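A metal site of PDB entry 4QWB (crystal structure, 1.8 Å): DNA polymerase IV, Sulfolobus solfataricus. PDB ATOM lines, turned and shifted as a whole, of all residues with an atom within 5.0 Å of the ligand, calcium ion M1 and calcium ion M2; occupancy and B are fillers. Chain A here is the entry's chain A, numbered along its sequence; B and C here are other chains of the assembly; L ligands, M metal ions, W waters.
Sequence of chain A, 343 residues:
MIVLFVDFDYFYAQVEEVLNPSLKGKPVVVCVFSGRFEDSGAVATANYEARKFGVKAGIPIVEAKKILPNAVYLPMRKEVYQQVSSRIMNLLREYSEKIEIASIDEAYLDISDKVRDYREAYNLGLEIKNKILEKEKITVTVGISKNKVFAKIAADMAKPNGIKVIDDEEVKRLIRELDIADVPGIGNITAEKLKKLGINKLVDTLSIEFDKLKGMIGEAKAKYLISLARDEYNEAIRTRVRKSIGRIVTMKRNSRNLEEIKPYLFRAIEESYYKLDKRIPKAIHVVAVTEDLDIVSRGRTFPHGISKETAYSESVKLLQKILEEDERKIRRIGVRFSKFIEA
Three residues have an atom within 4 Å of calcium ion M1: Asp 7, Phe 8 and Asp 105.
The backbone carbonyl oxygen (O) of Ala 44 sits close to a nitrogen (N2) of the ligand (3.5 Å).
Residues that only touch the ligand: Asp 9 (3.97 Å), Ala 57 (3.8 Å) and DG 6 of chain C (3.9 Å).
Of the 23 residues printed, 3 come within 4 Å of calcium ion M2.
Along chain A the residues within 4 Å of calcium ion M2 span positions 7 to 106.
The nearest printed residue that does not touch calcium ion M2 is Lys 159 (4.01 Å).
Water W3 bridges the side-chain amino group (NZ) of Lys 159 and an oxygen (O1) of the ligand.
Water W4 lies within hydrogen-bond range of NZ of Lys 159 and O6 of the ligand.
Water W9 lies within hydrogen-bond range of O1 of the ligand (2.7 Å), NH2 of Arg 51 (3.2 Å) and NZ of Lys 159 (3.3 Å).
Water W8 bridges O6 of the ligand (2.7 Å) and OP2 of DOC 13 of chain B (2.8 Å).
Water W5 lies within hydrogen-bond range of O10 of the ligand (2.8 Å), OH of Tyr 12 of chain A (2.8 Å) and N2 of DG 6 of chain C (3.3 Å).
Water W7 lies within hydrogen-bond range of the side-chain hydroxyl of Thr 45 (2.7 Å), the backbone carbonyl oxygen of Ala 44 (3.2 Å) and an oxygen (O4) of the ligand (3.3 Å).
OD2 of Asp 105 binds calcium ion M1.
An oxygen (O5) of the ligand binds calcium ion M1, at 2.2 Å.
Calcium ion M1 is bound by O2 of the ligand.
OD1 of Asp 7 is bound to calcium ion M1 (2.3 Å).
O of Phe 8 binds calcium ion M1 (2.3 Å).
Water W3 is bound to calcium ion M1, at 2.4 Å.
A nitrogen (N3) of the ligand lies within hydrogen-bond range of N4 of DOC 13 of chain B, 3.1 Å away.
O3 of the ligand is in hydrogen-bond range of OG1 of Thr 45, at 2.6 Å.
O6 of DG 5 of chain C lies within hydrogen-bond range of a nitrogen (N3) of the ligand.
NH2 of Arg 51 lies within salt-bridge range of O1 of the ligand, 3.0 Å away.
The backbone NH (N) of Phe 11 lies within hydrogen-bond range of an oxygen (O3) of the ligand, 3.3 Å away.
An oxygen (O9) of the ligand lies within hydrogen-bond range of the backbone NH (N) of Tyr 12 of chain A.
The backbone NH of Tyr 10 sits close to an oxygen (O2) of the ligand (3.3 Å).
The side-chain carboxylate (OD2) of Asp 7 binds calcium ion M2 (2.3 Å).
Water W10 binds calcium ion M2 (2.3 Å).
Water W1 binds calcium ion M2.
Calcium ion M2 is bound by OE2 of Glu 106.
OP1 of DOC 13 of chain B binds calcium ion M2 (2.3 Å).
Water W4 binds calcium ion M2, 2.4 Å away.
The side-chain carboxylate (OD2) of Asp 7 lies close to the side-chain amino group (NZ) of Lys 159 (3.0 Å).
OE2 of Glu 106 sits close to NZ of Lys 152 (3.3 Å).
O2 of DOC 13 of chain B sits close to N2 of DG 6 of chain C (2.6 Å).
The side-chain amino group of Lys 152 lies close to OP1 of DOC 13 of chain B.
OG1 of Thr 45 lies within hydrogen-bond range of NH1 of Arg 51.
The guanidinium group (NH1) of Arg 51 is in hydrogen-bond range of the backbone carbonyl oxygen (O) of Ala 46 (3.0 Å).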
ATOM      1  N   PHE A   5      12.966 -19.038  34.772  1.00  0.00           N
ATOM      2  CA  PHE A   5      11.848 -19.207  33.857  1.00  0.00           C
ATOM      3  C   PHE A   5      10.751 -18.208  34.223  1.00  0.00           C
ATOM      4  O   PHE A   5      10.435 -18.045  35.403  1.00  0.00           O
ATOM      5  CB  PHE A   5      11.345 -20.624  33.985  1.00  0.00           C
ATOM      6  CG  PHE A   5      10.041 -20.903  33.296  1.00  0.00           C
ATOM      7  CD1 PHE A   5       9.985 -21.077  31.908  1.00  0.00           C
ATOM      8  CD2 PHE A   5       8.867 -21.071  34.034  1.00  0.00           C
ATOM      9  CE1 PHE A   5       8.785 -21.362  31.288  1.00  0.00           C
ATOM     10  CE2 PHE A   5       7.675 -21.376  33.406  1.00  0.00           C
ATOM     11  CZ  PHE A   5       7.631 -21.517  32.026  1.00  0.00           C
ATOM     12  N   ASP A   7       6.703 -17.085  33.323  1.00  0.00           N
ATOM     13  CA  ASP A   7       5.458 -17.559  32.731  1.00  0.00           C
ATOM     14  C   ASP A   7       4.410 -16.500  33.091  1.00  0.00           C
ATOM     15  O   ASP A   7       4.182 -16.270  34.275  1.00  0.00           O
ATOM     16  CB  ASP A   7       5.095 -18.927  33.316  1.00  0.00           C
ATOM     17  CG  ASP A   7       3.837 -19.559  32.688  1.00  0.00           C
ATOM     18  OD1 ASP A   7       2.868 -18.853  32.362  1.00  0.00           O
ATOM     19  OD2 ASP A   7       3.779 -20.814  32.542  1.00  0.00           O
ATOM     20  N   PHE A   8       3.809 -15.837  32.109  1.00  0.00           N
ATOM     21  CA  PHE A   8       2.921 -14.692  32.400  1.00  0.00           C
ATOM     22  C   PHE A   8       1.604 -15.235  32.980  1.00  0.00           C
ATOM     23  O   PHE A   8       1.125 -16.254  32.513  1.00  0.00           O
ATOM     24  CB  PHE A   8       2.633 -13.797  31.165  1.00  0.00           C
ATOM     25  CG  PHE A   8       3.865 -13.409  30.362  1.00  0.00           C
ATOM     26  CD1 PHE A   8       5.125 -13.361  30.929  1.00  0.00           C
ATOM     27  CD2 PHE A   8       3.737 -13.053  29.017  1.00  0.00           C
ATOM     28  CE1 PHE A   8       6.233 -13.002  30.170  1.00  0.00           C
ATOM     29  CE2 PHE A   8       4.842 -12.684  28.258  1.00  0.00           C
ATOM     30  CZ  PHE A   8       6.088 -12.659  28.839  1.00  0.00           C
ATOM     31  N   ASP A   9       1.028 -14.562  33.983  1.00  0.00           N
ATOM     32  CA  ASP A   9      -0.221 -15.037  34.624  1.00  0.00           C
ATOM     33  C   ASP A   9      -1.457 -14.777  33.747  1.00  0.00           C
ATOM     34  O   ASP A   9      -1.576 -13.724  33.125  1.00  0.00           O
ATOM     35  CB  ASP A   9      -0.460 -14.348  35.976  1.00  0.00           C
ATOM     36  CG  ASP A   9       0.675 -14.555  36.992  1.00  0.00           C
ATOM     37  OD1 ASP A   9       1.217 -15.670  37.116  1.00  0.00           O
ATOM     38  OD2 ASP A   9       0.984 -13.589  37.718  1.00  0.00           O
ATOM     39  N   TYR A  10      -2.355 -15.769  33.700  1.00  0.00           N
ATOM     40  CA  TYR A  10      -3.659 -15.658  33.044  1.00  0.00           C
ATOM     41  C   TYR A  10      -3.584 -14.843  31.757  1.00  0.00           C
ATOM     42  O   TYR A  10      -4.415 -13.991  31.545  1.00  0.00           O
ATOM     43  CB  TYR A  10      -4.681 -15.007  34.016  1.00  0.00           C
ATOM     44  CG  TYR A  10      -4.829 -15.795  35.297  1.00  0.00           C
ATOM     45  CD1 TYR A  10      -5.443 -17.027  35.299  1.00  0.00           C
ATOM     46  CD2 TYR A  10      -4.319 -15.307  36.500  1.00  0.00           C
ATOM     47  CE1 TYR A  10      -5.568 -17.769  36.458  1.00  0.00           C
ATOM     48  CE2 TYR A  10      -4.438 -16.056  37.673  1.00  0.00           C
ATOM     49  CZ  TYR A  10      -5.056 -17.282  37.639  1.00  0.00           C
ATOM     50  OH  TYR A  10      -5.197 -18.059  38.777  1.00  0.00           O
ATOM     51  N   PHE A  11      -2.610 -15.138  30.895  1.00  0.00           N
ATOM     52  CA  PHE A  11      -2.064 -14.106  30.013  1.00  0.00           C
ATOM     53  C   PHE A  11      -3.059 -13.353  29.135  1.00  0.00           C
ATOM     54  O   PHE A  11      -3.140 -12.126  29.249  1.00  0.00           O
ATOM     55  CB  PHE A  11      -0.861 -14.611  29.181  1.00  0.00           C
ATOM     56  CG  PHE A  11      -0.215 -13.538  28.334  1.00  0.00           C
ATOM     57  CD1 PHE A  11       0.224 -12.345  28.909  1.00  0.00           C
ATOM     58  CD2 PHE A  11      -0.040 -13.709  26.972  1.00  0.00           C
ATOM     59  CE1 PHE A  11       0.800 -11.350  28.135  1.00  0.00           C
ATOM     60  CE2 PHE A  11       0.552 -12.722  26.195  1.00  0.00           C
ATOM     61  CZ  PHE A  11       0.970 -11.543  26.769  1.00  0.00           C
ATOM     62  N   TYR A  12      -3.823 -14.054  28.300  1.00  0.00           N
ATOM     63  CA  TYR A  12      -4.735 -13.349  27.398  1.00  0.00           C
ATOM     64  C   TYR A  12      -5.772 -12.543  28.170  1.00  0.00           C
ATOM     65  O   TYR A  12      -6.084 -11.415  27.797  1.00  0.00           O
ATOM     66  CB  TYR A  12      -5.476 -14.307  26.478  1.00  0.00           C
ATOM     67  CG  TYR A  12      -4.635 -14.996  25.427  1.00  0.00           C
ATOM     68  CD1 TYR A  12      -3.252 -14.832  25.356  1.00  0.00           C
ATOM     69  CD2 TYR A  12      -5.241 -15.877  24.528  1.00  0.00           C
ATOM     70  CE1 TYR A  12      -2.505 -15.502  24.380  1.00  0.00           C
ATOM     71  CE2 TYR A  12      -4.501 -16.558  23.570  1.00  0.00           C
ATOM     72  CZ  TYR A  12      -3.140 -16.346  23.499  1.00  0.00           C
ATOM     73  OH  TYR A  12      -2.414 -17.029  22.545  1.00  0.00           O
ATOM     74  N   ALA A  44     -10.170 -20.160  25.304  1.00  0.00           N
ATOM     75  CA  ALA A  44      -8.719 -20.078  25.188  1.00  0.00           C
ATOM     76  C   ALA A  44      -8.100 -19.996  26.566  1.00  0.00           C
ATOM     77  O   ALA A  44      -7.164 -20.720  26.874  1.00  0.00           O
ATOM     78  CB  ALA A  44      -8.327 -18.866  24.363  1.00  0.00           C
ATOM     79  N   THR A  45      -8.629 -19.093  27.395  1.00  0.00           N
ATOM     80  CA  THR A  45      -8.258 -19.032  28.807  1.00  0.00           C
ATOM     81  C   THR A  45      -9.295 -18.225  29.579  1.00  0.00           C
ATOM     82  O   THR A  45     -10.188 -17.625  29.016  1.00  0.00           O
ATOM     83  CB  THR A  45      -6.832 -18.441  29.011  1.00  0.00           C
ATOM     84  OG1 THR A  45      -6.317 -18.834  30.285  1.00  0.00           O
ATOM     85  CG2 THR A  45      -6.818 -16.918  28.900  1.00  0.00           C
ATOM     86  N   ALA A  46      -9.153 -18.233  30.906  1.00  0.00           N
ATOM     87  CA  ALA A  46      -9.983 -17.433  31.771  1.00  0.00           C
ATOM     88  C   ALA A  46      -9.130 -16.967  32.935  1.00  0.00           C
ATOM     89  O   ALA A  46      -8.121 -17.595  33.263  1.00  0.00           O
ATOM     90  CB  ALA A  46     -11.169 -18.244  32.267  1.00  0.00           C
ATOM     91  N   ARG A  51     -11.838 -19.078  36.521  1.00  0.00           N
ATOM     92  CA  ARG A  51     -11.208 -20.377  36.563  1.00  0.00           C
ATOM     93  C   ARG A  51     -11.478 -21.125  37.858  1.00  0.00           C
ATOM     94  O   ARG A  51     -11.594 -22.339  37.841  1.00  0.00           O
ATOM     95  CB  ARG A  51      -9.711 -20.266  36.313  1.00  0.00           C
ATOM     96  CG  ARG A  51      -9.212 -21.392  35.438  1.00  0.00           C
ATOM     97  CD  ARG A  51      -8.288 -20.876  34.364  1.00  0.00           C
ATOM     98  NE  ARG A  51      -6.922 -21.097  34.766  1.00  0.00           N
ATOM     99  CZ  ARG A  51      -5.851 -20.535  34.221  1.00  0.00           C
ATOM    100  NH1 ARG A  51      -5.947 -19.669  33.217  1.00  0.00           N
ATOM    101  NH2 ARG A  51      -4.671 -20.875  34.710  1.00  0.00           N
ATOM    102  N   ALA A  57      -9.303 -23.525  30.141  1.00  0.00           N
ATOM    103  CA  ALA A  57      -8.964 -23.610  28.724  1.00  0.00           C
ATOM    104  C   ALA A  57      -9.492 -24.894  28.097  1.00  0.00           C
ATOM    105  O   ALA A  57      -9.433 -25.969  28.708  1.00  0.00           O
ATOM    106  CB  ALA A  57      -7.461 -23.494  28.524  1.00  0.00           C
ATOM    107  N   GLY A  58     -10.022 -24.765  26.889  1.00  0.00           N
ATOM    108  CA  GLY A  58     -10.453 -25.929  26.125  1.00  0.00           C
ATOM    109  C   GLY A  58     -11.911 -26.296  26.263  1.00  0.00           C
ATOM    110  O   GLY A  58     -12.441 -26.968  25.376  1.00  0.00           O
ATOM    111  N   MET A  76     -10.990 -13.866  21.375  1.00  0.00           N
ATOM    112  CA  MET A  76      -9.539 -13.857  21.371  1.00  0.00           C
ATOM    113  C   MET A  76      -9.043 -12.843  20.358  1.00  0.00           C
ATOM    114  O   MET A  76      -9.520 -12.832  19.210  1.00  0.00           O
ATOM    115  CB  MET A  76      -9.010 -15.255  21.009  1.00  0.00           C
ATOM    116  CG  MET A  76      -7.528 -15.441  21.316  1.00  0.00           C
ATOM    117  SD  MET A  76      -6.955 -17.083  20.870  1.00  0.00           S
ATOM    118  CE  MET A  76      -7.082 -17.004  19.094  1.00  0.00           C
ATOM    119  N   ILE A 104       4.249 -17.857  23.606  1.00  0.00           N
ATOM    120  CA  ILE A 104       3.672 -16.521  23.664  1.00  0.00           C
ATOM    121  C   ILE A 104       3.794 -15.895  25.066  1.00  0.00           C
ATOM    122  O   ILE A 104       3.812 -14.670  25.190  1.00  0.00           O
ATOM    123  CB  ILE A 104       2.190 -16.500  23.193  1.00  0.00           C
ATOM    124  CG1 ILE A 104       1.743 -15.053  22.914  1.00  0.00           C
ATOM    125  CG2 ILE A 104       1.268 -17.225  24.182  1.00  0.00           C
ATOM    126  CD1 ILE A 104       0.535 -14.962  22.013  1.00  0.00           C
ATOM    127  N   ASP A 105       3.893 -16.717  26.107  1.00  0.00           N
ATOM    128  CA  ASP A 105       3.973 -16.173  27.472  1.00  0.00           C
ATOM    129  C   ASP A 105       5.094 -16.748  28.368  1.00  0.00           C
ATOM    130  O   ASP A 105       5.032 -16.617  29.586  1.00  0.00           O
ATOM    131  CB  ASP A 105       2.591 -16.261  28.153  1.00  0.00           C
ATOM    132  CG  ASP A 105       2.281 -17.654  28.676  1.00  0.00           C
ATOM    133  OD1 ASP A 105       2.783 -18.644  28.116  1.00  0.00           O
ATOM    134  OD2 ASP A 105       1.509 -17.742  29.663  1.00  0.00           O
ATOM    135  N   GLU A 106       6.132 -17.328  27.752  1.00  0.00           N
ATOM    136  CA  GLU A 106       7.214 -17.932  28.500  1.00  0.00           C
ATOM    137  C   GLU A 106       8.597 -17.630  27.940  1.00  0.00           C
ATOM    138  O   GLU A 106       8.799 -17.613  26.724  1.00  0.00           O
ATOM    139  CB  GLU A 106       7.090 -19.452  28.515  1.00  0.00           C
ATOM    140  CG  GLU A 106       5.860 -20.013  29.177  1.00  0.00           C
ATOM    141  CD  GLU A 106       5.671 -21.470  28.826  1.00  0.00           C
ATOM    142  OE1 GLU A 106       5.782 -21.805  27.619  1.00  0.00           O
ATOM    143  OE2 GLU A 106       5.398 -22.289  29.717  1.00  0.00           O
ATOM    144  N   LYS A 152      10.489 -24.714  35.218  1.00  0.00           N
ATOM    145  CA  LYS A 152       9.051 -24.694  34.897  1.00  0.00           C
ATOM    146  C   LYS A 152       8.209 -25.271  36.038  1.00  0.00           C
ATOM    147  O   LYS A 152       7.176 -24.689  36.394  1.00  0.00           O
ATOM    148  CB  LYS A 152       8.752 -25.466  33.598  1.00  0.00           C
ATOM    149  CG  LYS A 152       7.264 -25.576  33.292  1.00  0.00           C
ATOM    150  CD  LYS A 152       7.014 -26.123  31.901  1.00  0.00           C
ATOM    151  CE  LYS A 152       6.918 -25.026  30.846  1.00  0.00           C
ATOM    152  NZ  LYS A 152       6.094 -25.477  29.687  1.00  0.00           N
ATOM    153  N   LYS A 159       2.456 -20.371  41.037  1.00  0.00           N
ATOM    154  CA  LYS A 159       1.430 -19.611  40.336  1.00  0.00           C
ATOM    155  C   LYS A 159       0.213 -19.309  41.211  1.00  0.00           C
ATOM    156  O   LYS A 159      -0.219 -20.167  41.966  1.00  0.00           O
ATOM    157  CB  LYS A 159       0.916 -20.376  39.124  1.00  0.00           C
ATOM    158  CG  LYS A 159       1.798 -20.244  37.923  1.00  0.00           C
ATOM    159  CD  LYS A 159       1.223 -21.035  36.768  1.00  0.00           C
ATOM    160  CE  LYS A 159       2.218 -21.071  35.639  1.00  0.00           C
ATOM    161  NZ  LYS A 159       1.590 -21.662  34.436  1.00  0.00           N
ATOM    162  P    DT B  12       2.180 -31.573  28.553  1.00  0.00           P
ATOM    163  OP1  DT B  12       2.977 -31.539  29.800  1.00  0.00           O
ATOM    164  OP2  DT B  12       0.726 -31.801  28.629  1.00  0.00           O
ATOM    165  O5'  DT B  12       2.449 -30.217  27.766  1.00  0.00           O
ATOM    166  C5'  DT B  12       3.722 -29.562  27.841  1.00  0.00           C
ATOM    167  C4'  DT B  12       3.782 -28.377  26.910  1.00  0.00           C
ATOM    168  O4'  DT B  12       3.395 -28.761  25.572  1.00  0.00           O
ATOM    169  C3'  DT B  12       2.859 -27.226  27.239  1.00  0.00           C
ATOM    170  O3'  DT B  12       3.359 -26.395  28.285  1.00  0.00           O
ATOM    171  C2'  DT B  12       2.788 -26.492  25.914  1.00  0.00           C
ATOM    172  C1'  DT B  12       2.893 -27.619  24.888  1.00  0.00           C
ATOM    173  N1   DT B  12       1.613 -27.982  24.233  1.00  0.00           N
ATOM    174  C2   DT B  12       1.289 -27.322  23.073  1.00  0.00           C
ATOM    175  O2   DT B  12       2.011 -26.464  22.572  1.00  0.00           O
ATOM    176  N3   DT B  12       0.104 -27.703  22.505  1.00  0.00           N
ATOM    177  C4   DT B  12      -0.784 -28.644  22.981  1.00  0.00           C
ATOM    178  O4   DT B  12      -1.813 -28.898  22.354  1.00  0.00           O
ATOM    179  C5   DT B  12      -0.387 -29.295  24.215  1.00  0.00           C
ATOM    180  C7   DT B  12      -1.290 -30.332  24.817  1.00  0.00           C
ATOM    181  C6   DT B  12       0.767 -28.921  24.778  1.00  0.00           C
ATOM    182  N1  DOC B  13      -0.331 -23.926  24.472  1.00  0.00           N
ATOM    183  C2  DOC B  13      -1.278 -23.838  23.442  1.00  0.00           C
ATOM    184  N3  DOC B  13      -2.289 -24.739  23.392  1.00  0.00           N
ATOM    185  C4  DOC B  13      -2.363 -25.703  24.321  1.00  0.00           C
ATOM    186  C5  DOC B  13      -1.420 -25.799  25.383  1.00  0.00           C
ATOM    187  C6  DOC B  13      -0.427 -24.901  25.423  1.00  0.00           C
ATOM    188  O2  DOC B  13      -1.163 -22.943  22.591  1.00  0.00           O
ATOM    189  N4  DOC B  13      -3.374 -26.565  24.238  1.00  0.00           N
ATOM    190  C1' DOC B  13       0.766 -22.941  24.480  1.00  0.00           C
ATOM    191  C2' DOC B  13       0.455 -21.656  25.247  1.00  0.00           C
ATOM    192  C3' DOC B  13       1.223 -21.817  26.542  1.00  0.00           C
ATOM    193  C4' DOC B  13       2.421 -22.660  26.122  1.00  0.00           C
ATOM    194  O4' DOC B  13       1.897 -23.535  25.096  1.00  0.00           O
ATOM    195  C5' DOC B  13       3.024 -23.466  27.238  1.00  0.00           C
ATOM    196  O5' DOC B  13       2.040 -24.326  27.811  1.00  0.00           O
ATOM    197  P   DOC B  13       2.409 -25.312  28.999  1.00  0.00           P
ATOM    198  OP1 DOC B  13       3.225 -24.579  30.000  1.00  0.00           O
ATOM    199  OP2 DOC B  13       1.156 -25.979  29.392  1.00  0.00           O
ATOM    200  P    DG C   5     -13.358 -27.724  18.694  1.00  0.00           P
ATOM    201  OP1  DG C   5     -14.253 -27.863  17.515  1.00  0.00           O
ATOM    202  OP2  DG C   5     -12.212 -28.644  18.873  1.00  0.00           O
ATOM    203  O5'  DG C   5     -12.787 -26.242  18.732  1.00  0.00           O
ATOM    204  C5'  DG C   5     -13.649 -25.097  18.831  1.00  0.00           C
ATOM    205  C4'  DG C   5     -12.895 -23.874  18.357  1.00  0.00           C
ATOM    206  O4'  DG C   5     -11.981 -23.438  19.383  1.00  0.00           O
ATOM    207  C3'  DG C   5     -12.022 -24.112  17.131  1.00  0.00           C
ATOM    208  O3'  DG C   5     -11.919 -22.883  16.420  1.00  0.00           O
ATOM    209  C2'  DG C   5     -10.699 -24.560  17.743  1.00  0.00           C
ATOM    210  C1'  DG C   5     -10.634 -23.749  19.026  1.00  0.00           C
ATOM    211  N9   DG C   5     -10.017 -24.387  20.178  1.00  0.00           N
ATOM    212  C8   DG C   5     -10.372 -25.580  20.761  1.00  0.00           C
ATOM    213  N7   DG C   5      -9.679 -25.853  21.839  1.00  0.00           N
ATOM    214  C5   DG C   5      -8.840 -24.761  21.993  1.00  0.00           C
ATOM    215  C6   DG C   5      -7.873 -24.481  22.987  1.00  0.00           C
ATOM    216  O6   DG C   5      -7.546 -25.164  23.964  1.00  0.00           O
ATOM    217  N1   DG C   5      -7.253 -23.253  22.770  1.00  0.00           N
ATOM    218  C2   DG C   5      -7.536 -22.403  21.731  1.00  0.00           C
ATOM    219  N2   DG C   5      -6.831 -21.259  21.685  1.00  0.00           N
ATOM    220  N3   DG C   5      -8.446 -22.638  20.804  1.00  0.00           N
ATOM    221  C4   DG C   5      -9.056 -23.836  20.992  1.00  0.00           C
ATOM    222  P    DG C   6     -11.440 -22.868  14.901  1.00  0.00           P
ATOM    223  OP1  DG C   6     -11.904 -21.602  14.287  1.00  0.00           O
ATOM    224  OP2  DG C   6     -11.796 -24.181  14.289  1.00  0.00           O
ATOM    225  O5'  DG C   6      -9.873 -22.736  15.034  1.00  0.00           O
ATOM    226  C5'  DG C   6      -9.329 -21.477  15.417  1.00  0.00           C
ATOM    227  C4'  DG C   6      -7.920 -21.653  15.912  1.00  0.00           C
ATOM    228  O4'  DG C   6      -7.865 -22.505  17.066  1.00  0.00           O
ATOM    229  C3'  DG C   6      -6.951 -22.256  14.890  1.00  0.00           C
ATOM    230  O3'  DG C   6      -6.057 -21.175  14.639  1.00  0.00           O
ATOM    231  C2'  DG C   6      -6.351 -23.449  15.606  1.00  0.00           C
ATOM    232  C1'  DG C   6      -6.579 -23.056  17.058  1.00  0.00           C
ATOM    233  N9   DG C   6      -6.500 -24.086  18.094  1.00  0.00           N
ATOM    234  C8   DG C   6      -7.265 -25.223  18.243  1.00  0.00           C
ATOM    235  N7   DG C   6      -6.950 -25.912  19.305  1.00  0.00           N
ATOM    236  C5   DG C   6      -5.939 -25.184  19.900  1.00  0.00           C
ATOM    237  C6   DG C   6      -5.197 -25.430  21.087  1.00  0.00           C
ATOM    238  O6   DG C   6      -5.295 -26.378  21.865  1.00  0.00           O
ATOM    239  N1   DG C   6      -4.259 -24.426  21.328  1.00  0.00           N
ATOM    240  C2   DG C   6      -4.064 -23.329  20.527  1.00  0.00           C
ATOM    241  N2   DG C   6      -3.112 -22.464  20.921  1.00  0.00           N
ATOM    242  N3   DG C   6      -4.753 -23.078  19.428  1.00  0.00           N
ATOM    243  C4   DG C   6      -5.655 -24.045  19.173  1.00  0.00           C
HETATM  244  O1  LIG L   1      -2.993 -19.356  32.812  1.00  0.00           O
HETATM  245  P1  LIG L   1      -2.694 -18.792  31.436  1.00  0.00           P
HETATM  246  O2  LIG L   1      -1.455 -17.941  31.349  1.00  0.00           O
HETATM  247  O3  LIG L   1      -3.904 -18.141  30.813  1.00  0.00           O
HETATM  248  O4  LIG L   1      -2.495 -20.108  30.527  1.00  0.00           O
HETATM  249  P2  LIG L   1      -1.136 -20.788  29.984  1.00  0.00           P
HETATM  250  O5  LIG L   1       0.077 -20.327  30.741  1.00  0.00           O
HETATM  251  O6  LIG L   1      -1.448 -22.264  29.942  1.00  0.00           O
HETATM  252  O7  LIG L   1      -1.060 -20.338  28.446  1.00  0.00           O
HETATM  253  C1  LIG L   1      -0.738 -19.027  28.020  1.00  0.00           C
HETATM  254  C2  LIG L   1      -1.794 -18.516  27.055  1.00  0.00           C
HETATM  255  O8  LIG L   1      -1.859 -19.329  25.874  1.00  0.00           O
HETATM  256  C3  LIG L   1      -3.212 -18.479  27.605  1.00  0.00           C
HETATM  257  O9  LIG L   1      -3.464 -17.249  28.311  1.00  0.00           O
HETATM  258  C4  LIG L   1      -4.058 -18.623  26.362  1.00  0.00           C
HETATM  259  C5  LIG L   1      -3.187 -19.423  25.405  1.00  0.00           C
HETATM  260  N1  LIG L   1      -3.703 -20.777  25.448  1.00  0.00           N
HETATM  261  C6  LIG L   1      -4.681 -21.187  24.524  1.00  0.00           C
HETATM  262  O10 LIG L   1      -5.070 -20.416  23.641  1.00  0.00           O
HETATM  263  N2  LIG L   1      -5.190 -22.438  24.573  1.00  0.00           N
HETATM  264  C7  LIG L   1      -4.779 -23.300  25.535  1.00  0.00           C
HETATM  265  N3  LIG L   1      -5.285 -24.560  25.585  1.00  0.00           N
HETATM  266  C8  LIG L   1      -3.829 -22.906  26.454  1.00  0.00           C
HETATM  267  C9  LIG L   1      -3.303 -21.632  26.404  1.00  0.00           C
HETATM  268 CA    CA M   1       0.726 -18.379  31.637  1.00  0.00          CA
HETATM  269 CA    CA M   2       3.455 -22.477  30.976  1.00  0.00          CA
HETATM  270  O   HOH W   1       4.121 -23.900  32.684  1.00  0.00           O
HETATM  271  O   HOH W   2      -2.535 -23.475  32.349  1.00  0.00           O
HETATM  272  O   HOH W   3       0.291 -19.053  33.920  1.00  0.00           O
HETATM  273  O   HOH W   4       1.179 -22.643  31.843  1.00  0.00           O
HETATM  274  O   HOH W   5      -3.678 -19.292  21.516  1.00  0.00           O
HETATM  275  O   HOH W   6      -4.268 -25.970  27.993  1.00  0.00           O
HETATM  276  O   HOH W   7      -5.407 -21.197  29.445  1.00  0.00           O
HETATM  277  O   HOH W   8      -1.296 -24.739  28.768  1.00  0.00           O
HETATM  278  O   HOH W   9      -1.683 -21.434  33.865  1.00  0.00           O
HETATM  279  O   HOH W  10       2.410 -20.968  29.575  1.00  0.00           O
HETATM  280  O   HOH W  11      -1.886 -18.265  35.040  1.00  0.00           O
